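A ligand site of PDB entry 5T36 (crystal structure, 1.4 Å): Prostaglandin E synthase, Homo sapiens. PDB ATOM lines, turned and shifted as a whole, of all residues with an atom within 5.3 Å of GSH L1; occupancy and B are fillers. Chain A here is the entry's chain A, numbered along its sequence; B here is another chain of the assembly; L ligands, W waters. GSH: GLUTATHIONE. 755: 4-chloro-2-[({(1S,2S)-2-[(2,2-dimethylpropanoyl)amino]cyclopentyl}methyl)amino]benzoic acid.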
ATOM      1  N   ARG A  72      -8.341 -35.195  12.449  1.00  0.00           N
ATOM      2  CA  ARG A  72      -7.353 -34.358  11.767  1.00  0.00           C
ATOM      3  C   ARG A  72      -7.467 -32.883  12.167  1.00  0.00           C
ATOM      4  O   ARG A  72      -6.444 -32.221  12.372  1.00  0.00           O
ATOM      5  CB  ARG A  72      -7.478 -34.488  10.245  1.00  0.00           C
ATOM      6  CG  ARG A  72      -6.959 -35.814   9.697  1.00  0.00           C
ATOM      7  CD  ARG A  72      -6.725 -35.755   8.186  1.00  0.00           C
ATOM      8  NE  ARG A  72      -7.939 -35.518   7.415  1.00  0.00           N
ATOM      9  CZ  ARG A  72      -8.830 -36.460   7.089  1.00  0.00           C
ATOM     10  NH1 ARG A  72      -8.655 -37.714   7.479  1.00  0.00           N
ATOM     11  NH2 ARG A  72      -9.901 -36.136   6.375  1.00  0.00           N
ATOM     12  N   ALA A  73      -8.702 -32.394  12.273  1.00  0.00           N
ATOM     13  CA  ALA A  73      -8.943 -31.016  12.717  1.00  0.00           C
ATOM     14  C   ALA A  73      -8.450 -30.806  14.138  1.00  0.00           C
ATOM     15  O   ALA A  73      -7.802 -29.802  14.438  1.00  0.00           O
ATOM     16  CB  ALA A  73     -10.424 -30.673  12.599  1.00  0.00           C
ATOM     17  N   ARG A  75      -6.164 -32.643  15.685  1.00  0.00           N
ATOM     18  CA  ARG A  75      -4.707 -32.738  15.693  1.00  0.00           C
ATOM     19  C   ARG A  75      -4.058 -31.450  15.189  1.00  0.00           C
ATOM     20  O   ARG A  75      -3.084 -30.987  15.768  1.00  0.00           O
ATOM     21  CB  ARG A  75      -4.209 -33.953  14.896  1.00  0.00           C
ATOM     22  CG  ARG A  75      -2.710 -34.149  15.057  1.00  0.00           C
ATOM     23  CD  ARG A  75      -2.158 -35.263  14.204  1.00  0.00           C
ATOM     24  NE  ARG A  75      -0.747 -34.997  13.929  1.00  0.00           N
ATOM     25  CZ  ARG A  75       0.196 -35.929  13.793  1.00  0.00           C
ATOM     26  NH1 ARG A  75       1.438 -35.551  13.550  1.00  0.00           N
ATOM     27  NH2 ARG A  75      -0.098 -37.218  13.918  1.00  0.00           N
ATOM     28  N   ASN A  76      -4.615 -30.875  14.127  1.00  0.00           N
ATOM     29  CA  ASN A  76      -4.080 -29.616  13.615  1.00  0.00           C
ATOM     30  C   ASN A  76      -4.188 -28.502  14.656  1.00  0.00           C
ATOM     31  O   ASN A  76      -3.266 -27.693  14.799  1.00  0.00           O
ATOM     32  CB  ASN A  76      -4.745 -29.211  12.299  1.00  0.00           C
ATOM     33  CG  ASN A  76      -3.999 -28.090  11.598  1.00  0.00           C
ATOM     34  OD1 ASN A  76      -4.219 -26.908  11.888  1.00  0.00           O
ATOM     35  ND2 ASN A  76      -3.110 -28.448  10.679  1.00  0.00           N
ATOM     36  N   GLU A  79      -1.362 -28.943  16.928  1.00  0.00           N
ATOM     37  CA  GLU A  79      -0.130 -28.525  16.250  1.00  0.00           C
ATOM     38  C   GLU A  79       0.045 -27.010  16.198  1.00  0.00           C
ATOM     39  O   GLU A  79       1.154 -26.519  15.930  1.00  0.00           O
ATOM     40  CB  GLU A  79      -0.071 -29.125  14.842  1.00  0.00           C
ATOM     41  CG  GLU A  79       0.085 -30.647  14.813  1.00  0.00           C
ATOM     42  CD  GLU A  79      -0.042 -31.263  13.421  1.00  0.00           C
ATOM     43  OE1 GLU A  79      -0.318 -30.528  12.444  1.00  0.00           O
ATOM     44  OE2 GLU A  79       0.130 -32.485  13.304  1.00  0.00           O
ATOM     45  N   HIS A 115     -10.439 -22.018  10.270  1.00  0.00           N
ATOM     46  CA  HIS A 115      -9.797 -23.293   9.938  1.00  0.00           C
ATOM     47  C   HIS A 115     -10.697 -24.488  10.257  1.00  0.00           C
ATOM     48  O   HIS A 115     -10.849 -25.390   9.443  1.00  0.00           O
ATOM     49  CB  HIS A 115      -8.451 -23.427  10.641  1.00  0.00           C
ATOM     50  CG  HIS A 115      -7.670 -24.649  10.234  1.00  0.00           C
ATOM     51  ND1 HIS A 115      -7.854 -25.874  10.831  1.00  0.00           N
ATOM     52  CD2 HIS A 115      -6.718 -24.815   9.291  1.00  0.00           C
ATOM     53  CE1 HIS A 115      -7.036 -26.752  10.261  1.00  0.00           C
ATOM     54  NE2 HIS A 115      -6.336 -26.134   9.330  1.00  0.00           N
ATOM     55  N   TYR A 119     -12.420 -26.979   7.685  1.00  0.00           N
ATOM     56  CA  TYR A 119     -12.059 -28.390   7.759  1.00  0.00           C
ATOM     57  C   TYR A 119     -13.294 -29.275   7.916  1.00  0.00           C
ATOM     58  O   TYR A 119     -13.525 -30.161   7.093  1.00  0.00           O
ATOM     59  CB  TYR A 119     -11.079 -28.664   8.915  1.00  0.00           C
ATOM     60  CG  TYR A 119     -10.033 -29.706   8.574  1.00  0.00           C
ATOM     61  CD1 TYR A 119     -10.239 -30.623   7.544  1.00  0.00           C
ATOM     62  CD2 TYR A 119      -8.835 -29.771   9.290  1.00  0.00           C
ATOM     63  CE1 TYR A 119      -9.278 -31.563   7.222  1.00  0.00           C
ATOM     64  CE2 TYR A 119      -7.860 -30.722   8.976  1.00  0.00           C
ATOM     65  CZ  TYR A 119      -8.092 -31.610   7.936  1.00  0.00           C
ATOM     66  OH  TYR A 119      -7.157 -32.557   7.599  1.00  0.00           O
ATOM     67  N   ARG A 128      -8.993 -23.845   3.582  1.00  0.00           N
ATOM     68  CA  ARG A 128      -8.424 -24.319   4.852  1.00  0.00           C
ATOM     69  C   ARG A 128      -6.933 -24.001   4.963  1.00  0.00           C
ATOM     70  O   ARG A 128      -6.479 -23.517   5.996  1.00  0.00           O
ATOM     71  CB  ARG A 128      -8.663 -25.819   5.034  1.00  0.00           C
ATOM     72  CG  ARG A 128      -8.264 -26.349   6.407  1.00  0.00           C
ATOM     73  CD  ARG A 128      -8.051 -27.851   6.400  1.00  0.00           C
ATOM     74  NE  ARG A 128      -6.816 -28.249   5.716  1.00  0.00           N
ATOM     75  CZ  ARG A 128      -6.760 -28.834   4.528  1.00  0.00           C
ATOM     76  NH1 ARG A 128      -7.878 -29.116   3.862  1.00  0.00           N
ATOM     77  NH2 ARG A 128      -5.588 -29.154   4.010  1.00  0.00           N
ATOM     78  N   SER A 129      -6.189 -24.267   3.889  1.00  0.00           N
ATOM     79  CA  SER A 129      -4.744 -23.996   3.850  1.00  0.00           C
ATOM     80  C   SER A 129      -4.424 -22.518   4.077  1.00  0.00           C
ATOM     81  O   SER A 129      -3.456 -22.183   4.760  1.00  0.00           O
ATOM     82  CB  SER A 129      -4.141 -24.496   2.544  1.00  0.00           C
ATOM     83  OG  SER A 129      -4.296 -25.895   2.424  1.00  0.00           O
ATOM     84  N   TYR A 132      -4.995 -21.637   7.787  1.00  0.00           N
ATOM     85  CA  TYR A 132      -3.839 -22.133   8.534  1.00  0.00           C
ATOM     86  C   TYR A 132      -2.667 -21.153   8.444  1.00  0.00           C
ATOM     87  O   TYR A 132      -2.105 -20.769   9.466  1.00  0.00           O
ATOM     88  CB  TYR A 132      -3.395 -23.507   8.005  1.00  0.00           C
ATOM     89  CG  TYR A 132      -2.035 -23.941   8.503  1.00  0.00           C
ATOM     90  CD1 TYR A 132      -1.872 -24.522   9.761  1.00  0.00           C
ATOM     91  CD2 TYR A 132      -0.886 -23.747   7.721  1.00  0.00           C
ATOM     92  CE1 TYR A 132      -0.627 -24.912  10.229  1.00  0.00           C
ATOM     93  CE2 TYR A 132       0.373 -24.138   8.186  1.00  0.00           C
ATOM     94  CZ  TYR A 132       0.491 -24.713   9.434  1.00  0.00           C
ATOM     95  OH  TYR A 132       1.727 -25.104   9.891  1.00  0.00           O
ATOM     96  N   ALA B  33       6.103 -28.878  10.256  1.00  0.00           N
ATOM     97  CA  ALA B  33       4.794 -28.673   9.631  1.00  0.00           C
ATOM     98  C   ALA B  33       4.921 -28.264   8.168  1.00  0.00           C
ATOM     99  O   ALA B  33       4.208 -28.797   7.306  1.00  0.00           O
ATOM    100  CB  ALA B  33       3.986 -27.657  10.414  1.00  0.00           C
ATOM    101  N   ILE B  34       5.818 -27.316   7.889  1.00  0.00           N
ATOM    102  CA  ILE B  34       6.071 -26.850   6.524  1.00  0.00           C
ATOM    103  C   ILE B  34       6.616 -27.977   5.641  1.00  0.00           C
ATOM    104  O   ILE B  34       6.146 -28.184   4.523  1.00  0.00           O
ATOM    105  CB  ILE B  34       7.019 -25.617   6.507  1.00  0.00           C
ATOM    106  CG1 ILE B  34       6.329 -24.417   7.162  1.00  0.00           C
ATOM    107  CG2 ILE B  34       7.440 -25.273   5.074  1.00  0.00           C
ATOM    108  CD1 ILE B  34       7.286 -23.327   7.640  1.00  0.00           C
ATOM    109  N   THR B  36       6.178 -31.186   6.094  1.00  0.00           N
ATOM    110  CA  THR B  36       5.056 -32.110   5.882  1.00  0.00           C
ATOM    111  C   THR B  36       4.197 -31.688   4.687  1.00  0.00           C
ATOM    112  O   THR B  36       3.907 -32.511   3.810  1.00  0.00           O
ATOM    113  CB  THR B  36       4.171 -32.242   7.153  1.00  0.00           C
ATOM    114  OG1 THR B  36       4.991 -32.590   8.274  1.00  0.00           O
ATOM    115  CG2 THR B  36       3.113 -33.322   6.962  1.00  0.00           C
ATOM    116  N   GLY B  37       3.824 -30.411   4.648  1.00  0.00           N
ATOM    117  CA  GLY B  37       3.041 -29.858   3.543  1.00  0.00           C
ATOM    118  C   GLY B  37       3.737 -29.974   2.199  1.00  0.00           C
ATOM    119  O   GLY B  37       3.107 -30.342   1.195  1.00  0.00           O
ATOM    120  N   ARG B  40       3.750 -33.596   1.073  1.00  0.00           N
ATOM    121  CA  ARG B  40       2.404 -33.896   0.565  1.00  0.00           C
ATOM    122  C   ARG B  40       2.233 -33.454  -0.889  1.00  0.00           C
ATOM    123  O   ARG B  40       1.690 -34.197  -1.701  1.00  0.00           O
ATOM    124  CB  ARG B  40       1.328 -33.235   1.439  1.00  0.00           C
ATOM    125  CG  ARG B  40       1.090 -33.899   2.780  1.00  0.00           C
ATOM    126  CD  ARG B  40      -0.198 -33.391   3.413  1.00  0.00           C
ATOM    127  NE  ARG B  40      -0.488 -33.998   4.704  1.00  0.00           N
ATOM    128  CZ  ARG B  40      -1.074 -35.187   4.868  1.00  0.00           C
ATOM    129  NH1 ARG B  40      -1.424 -35.921   3.827  1.00  0.00           N
ATOM    130  NH2 ARG B  40      -1.306 -35.643   6.090  1.00  0.00           N
ATOM    131  N   ASN B  48      -7.137 -35.237   2.459  1.00  0.00           N
ATOM    132  CA  ASN B  48      -8.493 -34.759   2.206  1.00  0.00           C
ATOM    133  C   ASN B  48      -8.843 -34.777   0.719  1.00  0.00           C
ATOM    134  O   ASN B  48      -8.028 -34.363  -0.105  1.00  0.00           O
ATOM    135  CB  ASN B  48      -8.654 -33.343   2.754  1.00  0.00           C
ATOM    136  CG  ASN B  48      -8.326 -33.254   4.228  1.00  0.00           C
ATOM    137  OD1 ASN B  48      -8.999 -33.859   5.056  1.00  0.00           O
ATOM    138  ND2 ASN B  48      -7.291 -32.494   4.564  1.00  0.00           N
ATOM    139  N   LEU B  71       4.594 -36.902   9.959  1.00  0.00           N
ATOM    140  CA  LEU B  71       3.547 -36.841  10.976  1.00  0.00           C
ATOM    141  C   LEU B  71       3.983 -37.463  12.304  1.00  0.00           C
ATOM    142  O   LEU B  71       3.667 -36.938  13.362  1.00  0.00           O
ATOM    143  CB  LEU B  71       2.252 -37.494  10.486  1.00  0.00           C
ATOM    144  CG  LEU B  71       1.409 -36.724   9.461  1.00  0.00           C
ATOM    145  CD1 LEU B  71       0.347 -37.637   8.872  1.00  0.00           C
ATOM    146  CD2 LEU B  71       0.766 -35.481  10.066  1.00  0.00           C
ATOM    147  N   HIS B  74       6.414 -35.038  13.988  1.00  0.00           N
ATOM    148  CA  HIS B  74       5.626 -33.942  14.529  1.00  0.00           C
ATOM    149  C   HIS B  74       4.885 -34.363  15.793  1.00  0.00           C
ATOM    150  O   HIS B  74       4.850 -33.618  16.772  1.00  0.00           O
ATOM    151  CB  HIS B  74       4.625 -33.426  13.490  1.00  0.00           C
ATOM    152  CG  HIS B  74       4.177 -32.016  13.712  1.00  0.00           C
ATOM    153  ND1 HIS B  74       3.569 -31.267  12.730  1.00  0.00           N
ATOM    154  CD2 HIS B  74       4.263 -31.211  14.802  1.00  0.00           C
ATOM    155  CE1 HIS B  74       3.289 -30.064  13.203  1.00  0.00           C
ATOM    156  NE2 HIS B  74       3.700 -30.007  14.467  1.00  0.00           N
HETATM  157  N1  GSH L   1       0.226 -32.085  10.052  1.00  0.00           N
HETATM  158  CA1 GSH L   1      -0.092 -31.150   8.980  1.00  0.00           C
HETATM  159  C1  GSH L   1      -0.534 -31.906   7.757  1.00  0.00           C
HETATM  160  O11 GSH L   1      -1.157 -31.322   6.848  1.00  0.00           O
HETATM  161  O12 GSH L   1      -0.290 -33.130   7.635  1.00  0.00           O
HETATM  162  CB1 GSH L   1       1.135 -30.286   8.710  1.00  0.00           C
HETATM  163  CG1 GSH L   1       0.913 -29.156   7.709  1.00  0.00           C
HETATM  164  CD1 GSH L   1      -0.331 -28.355   8.002  1.00  0.00           C
HETATM  165  OE1 GSH L   1      -0.635 -27.952   9.309  1.00  0.00           O
HETATM  166  N2  GSH L   1      -1.107 -28.057   6.957  1.00  0.00           N
HETATM  167  CA2 GSH L   1      -2.341 -27.320   7.100  1.00  0.00           C
HETATM  168  C2  GSH L   1      -3.536 -28.200   7.364  1.00  0.00           C
HETATM  169  O2  GSH L   1      -4.796 -27.611   7.548  1.00  0.00           O
HETATM  170  CB2 GSH L   1      -2.584 -26.472   5.854  1.00  0.00           C
HETATM  171  SG2 GSH L   1      -2.563 -27.471   4.345  1.00  0.00           S
HETATM  172  N3  GSH L   1      -3.333 -29.515   7.408  1.00  0.00           N
HETATM  173  CA3 GSH L   1      -4.425 -30.457   7.601  1.00  0.00           C
HETATM  174  C3  GSH L   1      -4.195 -31.404   8.762  1.00  0.00           C
HETATM  175  O31 GSH L   1      -3.292 -31.177   9.609  1.00  0.00           O
HETATM  176  O32 GSH L   1      -4.909 -32.423   8.894  1.00  0.00           O
HETATM  177  O1  755 L   2      -2.881 -25.139  -3.065  1.00  0.00           O
HETATM  178  C7  755 L   2       0.558 -24.614   3.951  1.00  0.00           C
HETATM  179  O2  755 L   2      -2.712 -23.232  -4.250  1.00  0.00           O
HETATM  180  C6  755 L   2       1.554 -26.569   5.136  1.00  0.00           C
HETATM  181  C1  755 L   2      -1.831 -29.339   0.873  1.00  0.00           C
HETATM  182  N1  755 L   2      -1.602 -25.128  -0.702  1.00  0.00           N
HETATM  183  C5  755 L   2       1.701 -25.645   3.913  1.00  0.00           C
HETATM  184  C4  755 L   2       1.648 -26.452   2.594  1.00  0.00           C
HETATM  185  C3  755 L   2       0.194 -27.966   1.214  1.00  0.00           C
HETATM  186  C2  755 L   2      -0.496 -29.277   1.616  1.00  0.00           C
HETATM  187 CL   755 L   2      -1.596 -20.700   1.848  1.00  0.00          CL
HETATM  188  C13 755 L   2      -1.897 -21.620   0.427  1.00  0.00           C
HETATM  189  C14 755 L   2      -2.403 -20.987  -0.719  1.00  0.00           C
HETATM  190  C12 755 L   2      -1.631 -22.985   0.414  1.00  0.00           C
HETATM  191  C11 755 L   2      -1.874 -23.750  -0.735  1.00  0.00           C
HETATM  192  C16 755 L   2      -2.381 -23.125  -1.887  1.00  0.00           C
HETATM  193  C17 755 L   2      -2.661 -23.872  -3.140  1.00  0.00           C
HETATM  194  C15 755 L   2      -2.645 -21.753  -1.868  1.00  0.00           C
HETATM  195  C10 755 L   2      -0.744 -25.749   0.254  1.00  0.00           C
HETATM  196  C9  755 L   2      -0.765 -27.277   0.210  1.00  0.00           C
HETATM  197  C   755 L   2      -2.138 -27.885   0.496  1.00  0.00           C
HETATM  198  N   755 L   2       0.460 -27.156   2.382  1.00  0.00           N
HETATM  199  O   755 L   2       2.580 -26.466   1.794  1.00  0.00           O
HETATM  200  C8  755 L   2       3.026 -24.870   4.029  1.00  0.00           C
HETATM  201  O   HOH W   1      -3.356 -33.034   5.781  1.00  0.00           O
HETATM  202  O   HOH W   2      -2.387 -30.872   4.433  1.00  0.00           O
HETATM  203  O   HOH W   3       0.591 -28.115  11.656  1.00  0.00           O
HETATM  204  O   HOH W   4      -3.408 -34.707   7.866  1.00  0.00           O
HETATM  205  O   HOH W   5       2.934 -32.666  10.387  1.00  0.00           O
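The side-chain hydroxyl of Tyr 119 is in hydrogen-bond range of an oxygen (O32) of GSH L1 (2.6 Å).
An oxygen (O2) of GSH L1 lies within hydrogen-bond range of a ring nitrogen (NE2) of His 115 (2.8 Å).
The guanidinium group (NE) of Arg 128 is in hydrogen-bond range of an oxygen (O2) of GSH L1.
ND2 of Asn 76 lies within hydrogen-bond range of OE1 of GSH L1, 2.9 Å away.
The side-chain carboxylate of Glu 79 is in salt-bridge range of a nitrogen (N1) of GSH L1, 2.9 Å away.
The side-chain hydroxyl of Ser 129 sits close to a sulfur (SG2) of GSH L1 (3.0 Å).
The guanidinium group (NE) of Arg 40 of chain B is in salt-bridge range of an oxygen (O12) of GSH L1.
SG2 of GSH L1 sits close to N of 755 L2, at 3.6 Å.
OH of Tyr 119 lies within hydrogen-bond range of NE of Arg 72, at 3.1 Å.
The side-chain amide nitrogen (ND2) of Asn 48 of chain B sits at hydrogen-bond distance from the side-chain hydroxyl (OH) of Tyr 119 (3.0 Å).
NE2 of His 115 sits close to OD1 of Asn 76, 3.4 Å away.
NE of Arg 75 lies within salt-bridge range of OE2 of Glu 79 (2.7 Å).
The backbone carbonyl oxygen (O) of Leu 71 of chain B sits at hydrogen-bond distance from the guanidinium group (NH1) of Arg 75 (2.6 Å).
NH2 of Arg 72 lies within hydrogen-bond range of OD1 of Asn 48 of chain B (2.8 Å).
Merely in contact with GSH L1: Tyr 132 (3.2 Å), Ala 33 of chain B (3.3 Å), Leu 71 of chain B (3.4 Å), Thr 36 of chain B (3.5 Å) and Arg 72 (3.6 Å).
The nearest printed residue that does not touch GSH L1 is His 74 of chain B (4.4 Å).
Water W3 lies within hydrogen-bond range of OE1 of GSH L1 (2.7 Å) and OE1 of Glu 79 (2.7 Å).
Water W5 lies within hydrogen-bond range of N1 of GSH L1, ND1 of His 74 of chain B and OG1 of Thr 36 of chain B.
Water W4 bridges the guanidinium group (NH2) of Arg 40 of chain B (2.9 Å) and an oxygen (O32) of GSH L1 (2.9 Å).
Water W1 lies within hydrogen-bond range of O11 of GSH L1 and NE of Arg 40 of chain B.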
